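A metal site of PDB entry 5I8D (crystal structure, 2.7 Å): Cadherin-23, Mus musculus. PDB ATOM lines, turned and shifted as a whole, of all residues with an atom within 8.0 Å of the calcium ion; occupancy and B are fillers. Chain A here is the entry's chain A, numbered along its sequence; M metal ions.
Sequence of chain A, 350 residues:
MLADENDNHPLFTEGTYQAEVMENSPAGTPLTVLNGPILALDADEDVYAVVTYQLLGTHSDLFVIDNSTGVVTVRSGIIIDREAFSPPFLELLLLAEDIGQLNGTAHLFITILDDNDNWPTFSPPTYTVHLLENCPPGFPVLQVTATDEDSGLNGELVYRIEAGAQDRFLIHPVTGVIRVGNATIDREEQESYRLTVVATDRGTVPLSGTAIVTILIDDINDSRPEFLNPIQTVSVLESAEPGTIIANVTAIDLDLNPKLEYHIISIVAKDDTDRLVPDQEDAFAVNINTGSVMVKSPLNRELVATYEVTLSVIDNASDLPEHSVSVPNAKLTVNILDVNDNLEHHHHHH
The side-chain amide oxygen (OD1) of Asn 6 binds the calcium ion. The side-chain carboxylate (OD2) of Asp 98 is bound to the calcium ion, 2.4 Å away. OD2 of Asp 44 binds the calcium ion. The calcium ion is bound by O of Asn 8. The calcium ion is bound by O of Tyr 48 (2.5 Å). OD2 of Asp 42 is bound to the calcium ion (2.6 Å). The calcium ion is bound by OD1 of Asp 42. The calcium ion has seven donor atoms within binding distance.
Of the 24 residues printed, 6 come within 4 Å of the calcium ion. The nearest printed residue that does not touch the calcium ion is His 9 (4.2 Å).
N of Leu 102 lies within hydrogen-bond range of OD1 of Asp 98. The side-chain carboxylate (OD1) of Asp 44 is in hydrogen-bond range of the backbone NH (N) of Asp 7, at 2.9 Å. OD1 of Asp 98 sits at hydrogen-bond distance from N of Gly 100 (3.1 Å). The backbone NH (N) of Gln 101 lies within hydrogen-bond range of the side-chain carboxylate (OD1) of Asp 98, at 3.1 Å.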
ATOM      1  N   GLU A   5      -0.137  -2.763 -19.756  1.00  0.00           N
ATOM      2  CA  GLU A   5       1.208  -2.112 -19.611  1.00  0.00           C
ATOM      3  C   GLU A   5       2.266  -2.676 -20.579  1.00  0.00           C
ATOM      4  O   GLU A   5       2.062  -3.736 -21.205  1.00  0.00           O
ATOM      5  CB  GLU A   5       1.730  -2.151 -18.148  1.00  0.00           C
ATOM      6  CG  GLU A   5       1.313  -0.936 -17.293  1.00  0.00           C
ATOM      7  CD  GLU A   5       2.236   0.293 -17.463  1.00  0.00           C
ATOM      8  OE1 GLU A   5       2.667   0.832 -16.425  1.00  0.00           O
ATOM      9  OE2 GLU A   5       2.538   0.738 -18.605  1.00  0.00           O
ATOM     10  N   ASN A   6       3.369  -1.949 -20.701  1.00  0.00           N
ATOM     11  CA  ASN A   6       4.469  -2.267 -21.621  1.00  0.00           C
ATOM     12  C   ASN A   6       5.670  -2.825 -20.817  1.00  0.00           C
ATOM     13  O   ASN A   6       6.661  -2.115 -20.569  1.00  0.00           O
ATOM     14  CB  ASN A   6       4.818  -0.995 -22.434  1.00  0.00           C
ATOM     15  CG  ASN A   6       5.630  -1.289 -23.695  1.00  0.00           C
ATOM     16  OD1 ASN A   6       5.552  -2.368 -24.279  1.00  0.00           O
ATOM     17  ND2 ASN A   6       6.387  -0.314 -24.137  1.00  0.00           N
ATOM     18  N   ASP A   7       5.575  -4.088 -20.417  1.00  0.00           N
ATOM     19  CA  ASP A   7       6.587  -4.740 -19.547  1.00  0.00           C
ATOM     20  C   ASP A   7       7.779  -5.359 -20.302  1.00  0.00           C
ATOM     21  O   ASP A   7       8.725  -5.825 -19.667  1.00  0.00           O
ATOM     22  CB  ASP A   7       5.926  -5.820 -18.647  1.00  0.00           C
ATOM     23  CG  ASP A   7       4.904  -5.239 -17.649  1.00  0.00           C
ATOM     24  OD1 ASP A   7       5.266  -4.346 -16.831  1.00  0.00           O
ATOM     25  OD2 ASP A   7       3.742  -5.699 -17.668  1.00  0.00           O
ATOM     26  N   ASN A   8       7.722  -5.387 -21.632  1.00  0.00           N
ATOM     27  CA  ASN A   8       8.770  -5.997 -22.483  1.00  0.00           C
ATOM     28  C   ASN A   8       9.030  -5.172 -23.729  1.00  0.00           C
ATOM     29  O   ASN A   8       8.226  -4.312 -24.112  1.00  0.00           O
ATOM     30  CB  ASN A   8       8.362  -7.395 -22.970  1.00  0.00           C
ATOM     31  CG  ASN A   8       8.042  -8.345 -21.856  1.00  0.00           C
ATOM     32  OD1 ASN A   8       8.850  -9.207 -21.522  1.00  0.00           O
ATOM     33  ND2 ASN A   8       6.843  -8.231 -21.297  1.00  0.00           N
ATOM     34  N   HIS A   9      10.130  -5.482 -24.396  1.00  0.00           N
ATOM     35  CA  HIS A   9      10.516  -4.794 -25.626  1.00  0.00           C
ATOM     36  C   HIS A   9      10.779  -5.835 -26.717  1.00  0.00           C
ATOM     37  O   HIS A   9      10.912  -7.042 -26.432  1.00  0.00           O
ATOM     38  CB  HIS A   9      11.745  -3.919 -25.363  1.00  0.00           C
ATOM     39  CG  HIS A   9      12.950  -4.704 -24.944  1.00  0.00           C
ATOM     40  ND1 HIS A   9      13.869  -5.190 -25.855  1.00  0.00           N
ATOM     41  CD2 HIS A   9      13.361  -5.109 -23.727  1.00  0.00           C
ATOM     42  CE1 HIS A   9      14.810  -5.848 -25.199  1.00  0.00           C
ATOM     43  NE2 HIS A   9      14.522  -5.820 -23.917  1.00  0.00           N
ATOM     44  N   PRO A  10      10.840  -5.377 -27.995  1.00  0.00           N
ATOM     45  CA  PRO A  10      11.099  -6.312 -29.080  1.00  0.00           C
ATOM     46  C   PRO A  10      12.470  -6.983 -28.988  1.00  0.00           C
ATOM     47  O   PRO A  10      13.443  -6.378 -28.498  1.00  0.00           O
ATOM     48  CB  PRO A  10      11.006  -5.431 -30.350  1.00  0.00           C
ATOM     49  CG  PRO A  10      10.241  -4.222 -29.937  1.00  0.00           C
ATOM     50  CD  PRO A  10      10.634  -3.995 -28.512  1.00  0.00           C
ATOM     51  N   LEU A  41      10.170 -10.374 -31.868  1.00  0.00           N
ATOM     52  CA  LEU A  41       9.001 -10.685 -31.063  1.00  0.00           C
ATOM     53  C   LEU A  41       8.988  -9.839 -29.789  1.00  0.00           C
ATOM     54  O   LEU A  41      10.033  -9.494 -29.260  1.00  0.00           O
ATOM     55  CB  LEU A  41       8.992 -12.178 -30.756  1.00  0.00           C
ATOM     56  CG  LEU A  41       8.820 -13.045 -32.013  1.00  0.00           C
ATOM     57  CD1 LEU A  41       9.387 -14.453 -31.823  1.00  0.00           C
ATOM     58  CD2 LEU A  41       7.359 -13.119 -32.437  1.00  0.00           C
ATOM     59  N   ASP A  42       7.798  -9.480 -29.332  1.00  0.00           N
ATOM     60  CA  ASP A  42       7.599  -8.680 -28.138  1.00  0.00           C
ATOM     61  C   ASP A  42       6.589  -9.394 -27.256  1.00  0.00           C
ATOM     62  O   ASP A  42       5.462  -9.645 -27.673  1.00  0.00           O
ATOM     63  CB  ASP A  42       7.111  -7.301 -28.523  1.00  0.00           C
ATOM     64  CG  ASP A  42       7.059  -6.331 -27.360  1.00  0.00           C
ATOM     65  OD1 ASP A  42       6.389  -6.581 -26.344  1.00  0.00           O
ATOM     66  OD2 ASP A  42       7.639  -5.253 -27.500  1.00  0.00           O
ATOM     67  N   ALA A  43       6.998  -9.709 -26.023  1.00  0.00           N
ATOM     68  CA  ALA A  43       6.259 -10.596 -25.126  1.00  0.00           C
ATOM     69  C   ALA A  43       5.001 -10.009 -24.464  1.00  0.00           C
ATOM     70  O   ALA A  43       4.261 -10.771 -23.828  1.00  0.00           O
ATOM     71  CB  ALA A  43       7.194 -11.169 -24.057  1.00  0.00           C
ATOM     72  N   ASP A  44       4.742  -8.707 -24.604  1.00  0.00           N
ATOM     73  CA  ASP A  44       3.505  -8.089 -24.106  1.00  0.00           C
ATOM     74  C   ASP A  44       2.241  -8.595 -24.826  1.00  0.00           C
ATOM     75  O   ASP A  44       2.329  -9.270 -25.842  1.00  0.00           O
ATOM     76  CB  ASP A  44       3.551  -6.555 -24.225  1.00  0.00           C
ATOM     77  CG  ASP A  44       4.570  -5.929 -23.282  1.00  0.00           C
ATOM     78  OD1 ASP A  44       4.506  -6.194 -22.056  1.00  0.00           O
ATOM     79  OD2 ASP A  44       5.442  -5.180 -23.782  1.00  0.00           O
ATOM     80  N   GLU A  45       1.083  -8.272 -24.259  1.00  0.00           N
ATOM     81  CA  GLU A  45      -0.208  -8.623 -24.845  1.00  0.00           C
ATOM     82  C   GLU A  45      -0.680  -7.447 -25.726  1.00  0.00           C
ATOM     83  O   GLU A  45      -0.413  -6.276 -25.396  1.00  0.00           O
ATOM     84  CB  GLU A  45      -1.271  -8.923 -23.739  1.00  0.00           C
ATOM     85  CG  GLU A  45      -0.778  -9.596 -22.440  1.00  0.00           C
ATOM     86  CD  GLU A  45      -1.874 -10.403 -21.711  1.00  0.00           C
ATOM     87  OE1 GLU A  45      -2.204 -10.103 -20.532  1.00  0.00           O
ATOM     88  OE2 GLU A  45      -2.414 -11.360 -22.320  1.00  0.00           O
ATOM     89  N   ASP A  46      -1.354  -7.753 -26.854  1.00  0.00           N
ATOM     90  CA  ASP A  46      -2.100  -6.755 -27.655  1.00  0.00           C
ATOM     91  C   ASP A  46      -1.228  -5.606 -28.237  1.00  0.00           C
ATOM     92  O   ASP A  46      -0.141  -5.861 -28.768  1.00  0.00           O
ATOM     93  CB  ASP A  46      -3.268  -6.180 -26.822  1.00  0.00           C
ATOM     94  CG  ASP A  46      -4.120  -7.245 -26.186  1.00  0.00           C
ATOM     95  OD1 ASP A  46      -3.800  -7.673 -25.051  1.00  0.00           O
ATOM     96  OD2 ASP A  46      -5.142  -7.609 -26.806  1.00  0.00           O
ATOM     97  N   VAL A  47      -1.709  -4.357 -28.106  1.00  0.00           N
ATOM     98  CA  VAL A  47      -1.113  -3.145 -28.694  1.00  0.00           C
ATOM     99  C   VAL A  47       0.380  -2.943 -28.357  1.00  0.00           C
ATOM    100  O   VAL A  47       1.145  -2.441 -29.187  1.00  0.00           O
ATOM    101  CB  VAL A  47      -1.944  -1.885 -28.285  1.00  0.00           C
ATOM    102  CG1 VAL A  47      -1.778  -1.526 -26.809  1.00  0.00           C
ATOM    103  CG2 VAL A  47      -1.616  -0.694 -29.189  1.00  0.00           C
ATOM    104  N   TYR A  48       0.784  -3.356 -27.172  1.00  0.00           N
ATOM    105  CA  TYR A  48       2.180  -3.231 -26.751  1.00  0.00           C
ATOM    106  C   TYR A  48       3.096  -4.346 -27.331  1.00  0.00           C
ATOM    107  O   TYR A  48       4.303  -4.382 -27.029  1.00  0.00           O
ATOM    108  CB  TYR A  48       2.263  -3.159 -25.213  1.00  0.00           C
ATOM    109  CG  TYR A  48       1.393  -2.064 -24.621  1.00  0.00           C
ATOM    110  CD1 TYR A  48       1.726  -0.707 -24.776  1.00  0.00           C
ATOM    111  CD2 TYR A  48       0.214  -2.384 -23.927  1.00  0.00           C
ATOM    112  CE1 TYR A  48       0.921   0.298 -24.245  1.00  0.00           C
ATOM    113  CE2 TYR A  48      -0.600  -1.386 -23.404  1.00  0.00           C
ATOM    114  CZ  TYR A  48      -0.253  -0.053 -23.557  1.00  0.00           C
ATOM    115  OH  TYR A  48      -1.059   0.933 -23.033  1.00  0.00           O
ATOM    116  N   ALA A  49       2.519  -5.231 -28.168  1.00  0.00           N
ATOM    117  CA  ALA A  49       3.253  -6.346 -28.784  1.00  0.00           C
ATOM    118  C   ALA A  49       3.652  -6.148 -30.255  1.00  0.00           C
ATOM    119  O   ALA A  49       4.529  -6.877 -30.734  1.00  0.00           O
ATOM    120  CB  ALA A  49       2.459  -7.639 -28.648  1.00  0.00           C
ATOM    121  N   VAL A  50       3.023  -5.192 -30.950  1.00  0.00           N
ATOM    122  CA  VAL A  50       3.297  -5.002 -32.396  1.00  0.00           C
ATOM    123  C   VAL A  50       4.534  -4.168 -32.605  1.00  0.00           C
ATOM    124  O   VAL A  50       4.710  -3.143 -31.909  1.00  0.00           O
ATOM    125  CB  VAL A  50       2.128  -4.374 -33.194  1.00  0.00           C
ATOM    126  CG1 VAL A  50       0.888  -5.253 -33.089  1.00  0.00           C
ATOM    127  CG2 VAL A  50       1.820  -2.939 -32.757  1.00  0.00           C
ATOM    128  N   VAL A  51       5.365  -4.587 -33.555  1.00  0.00           N
ATOM    129  CA  VAL A  51       6.673  -3.967 -33.760  1.00  0.00           C
ATOM    130  C   VAL A  51       6.722  -3.169 -35.073  1.00  0.00           C
ATOM    131  O   VAL A  51       6.141  -3.598 -36.078  1.00  0.00           O
ATOM    132  CB  VAL A  51       7.840  -4.988 -33.659  1.00  0.00           C
ATOM    133  CG1 VAL A  51       7.657  -5.903 -32.452  1.00  0.00           C
ATOM    134  CG2 VAL A  51       7.990  -5.838 -34.903  1.00  0.00           C
ATOM    135  N   GLU A  97      11.005  -1.430 -32.969  1.00  0.00           N
ATOM    136  CA  GLU A  97      10.382  -0.573 -31.922  1.00  0.00           C
ATOM    137  C   GLU A  97       8.977  -1.056 -31.575  1.00  0.00           C
ATOM    138  O   GLU A  97       8.315  -1.694 -32.414  1.00  0.00           O
ATOM    139  CB  GLU A  97      10.258   0.881 -32.396  1.00  0.00           C
ATOM    140  CG  GLU A  97      11.548   1.534 -32.842  1.00  0.00           C
ATOM    141  CD  GLU A  97      11.790   2.881 -32.158  1.00  0.00           C
ATOM    142  OE1 GLU A  97      11.999   3.901 -32.874  1.00  0.00           O
ATOM    143  OE2 GLU A  97      11.749   2.908 -30.909  1.00  0.00           O
ATOM    144  N   ASP A  98       8.508  -0.722 -30.367  1.00  0.00           N
ATOM    145  CA  ASP A  98       7.084  -0.890 -29.992  1.00  0.00           C
ATOM    146  C   ASP A  98       6.401   0.474 -29.799  1.00  0.00           C
ATOM    147  O   ASP A  98       7.057   1.517 -29.924  1.00  0.00           O
ATOM    148  CB  ASP A  98       6.939  -1.813 -28.774  1.00  0.00           C
ATOM    149  CG  ASP A  98       7.232  -1.114 -27.426  1.00  0.00           C
ATOM    150  OD1 ASP A  98       7.481   0.123 -27.338  1.00  0.00           O
ATOM    151  OD2 ASP A  98       7.218  -1.842 -26.405  1.00  0.00           O
ATOM    152  N   ILE A  99       5.096   0.467 -29.479  1.00  0.00           N
ATOM    153  CA  ILE A  99       4.282   1.711 -29.440  1.00  0.00           C
ATOM    154  C   ILE A  99       4.715   2.728 -28.382  1.00  0.00           C
ATOM    155  O   ILE A  99       4.596   3.942 -28.605  1.00  0.00           O
ATOM    156  CB  ILE A  99       2.755   1.405 -29.320  1.00  0.00           C
ATOM    157  CG1 ILE A  99       1.896   2.635 -29.668  1.00  0.00           C
ATOM    158  CG2 ILE A  99       2.366   0.932 -27.920  1.00  0.00           C
ATOM    159  CD1 ILE A  99       2.220   3.299 -31.013  1.00  0.00           C
ATOM    160  N   GLY A 100       5.228   2.251 -27.256  1.00  0.00           N
ATOM    161  CA  GLY A 100       5.883   3.099 -26.264  1.00  0.00           C
ATOM    162  C   GLY A 100       7.352   3.344 -26.545  1.00  0.00           C
ATOM    163  O   GLY A 100       8.109   3.648 -25.624  1.00  0.00           O
ATOM    164  N   GLN A 101       7.773   3.209 -27.808  1.00  0.00           N
ATOM    165  CA  GLN A 101       9.149   3.463 -28.276  1.00  0.00           C
ATOM    166  C   GLN A 101      10.267   2.753 -27.478  1.00  0.00           C
ATOM    167  O   GLN A 101      11.368   3.283 -27.377  1.00  0.00           O
ATOM    168  CB  GLN A 101       9.382   4.992 -28.431  1.00  0.00           C
ATOM    169  CG  GLN A 101       8.569   5.677 -29.543  1.00  0.00           C
ATOM    170  CD  GLN A 101       9.141   5.462 -30.968  1.00  0.00           C
ATOM    171  OE1 GLN A 101       8.577   4.720 -31.787  1.00  0.00           O
ATOM    172  NE2 GLN A 101      10.270   6.113 -31.260  1.00  0.00           N
ATOM    173  N   LEU A 102       9.985   1.574 -26.915  1.00  0.00           N
ATOM    174  CA  LEU A 102      11.013   0.645 -26.439  1.00  0.00           C
ATOM    175  C   LEU A 102      11.413  -0.173 -27.639  1.00  0.00           C
ATOM    176  O   LEU A 102      10.630  -0.279 -28.589  1.00  0.00           O
ATOM    177  CB  LEU A 102      10.484  -0.306 -25.381  1.00  0.00           C
ATOM    178  CG  LEU A 102       9.822   0.295 -24.142  1.00  0.00           C
ATOM    179  CD1 LEU A 102       9.427  -0.853 -23.220  1.00  0.00           C
ATOM    180  CD2 LEU A 102      10.737   1.286 -23.415  1.00  0.00           C
ATOM    181  N   ASN A 103      12.605  -0.760 -27.605  1.00  0.00           N
ATOM    182  CA  ASN A 103      13.213  -1.285 -28.830  1.00  0.00           C
ATOM    183  C   ASN A 103      14.149  -2.499 -28.649  1.00  0.00           C
ATOM    184  O   ASN A 103      14.453  -2.899 -27.554  1.00  0.00           O
ATOM    185  CB  ASN A 103      13.957  -0.152 -29.556  1.00  0.00           C
ATOM    186  CG  ASN A 103      15.254   0.247 -28.849  1.00  0.00           C
ATOM    187  OD1 ASN A 103      16.181  -0.550 -28.788  1.00  0.00           O
ATOM    188  ND2 ASN A 103      15.303   1.463 -28.303  1.00  0.00           N
HETATM  189 CA    CA M   1       6.374  -3.956 -25.631  1.00  0.00          CA
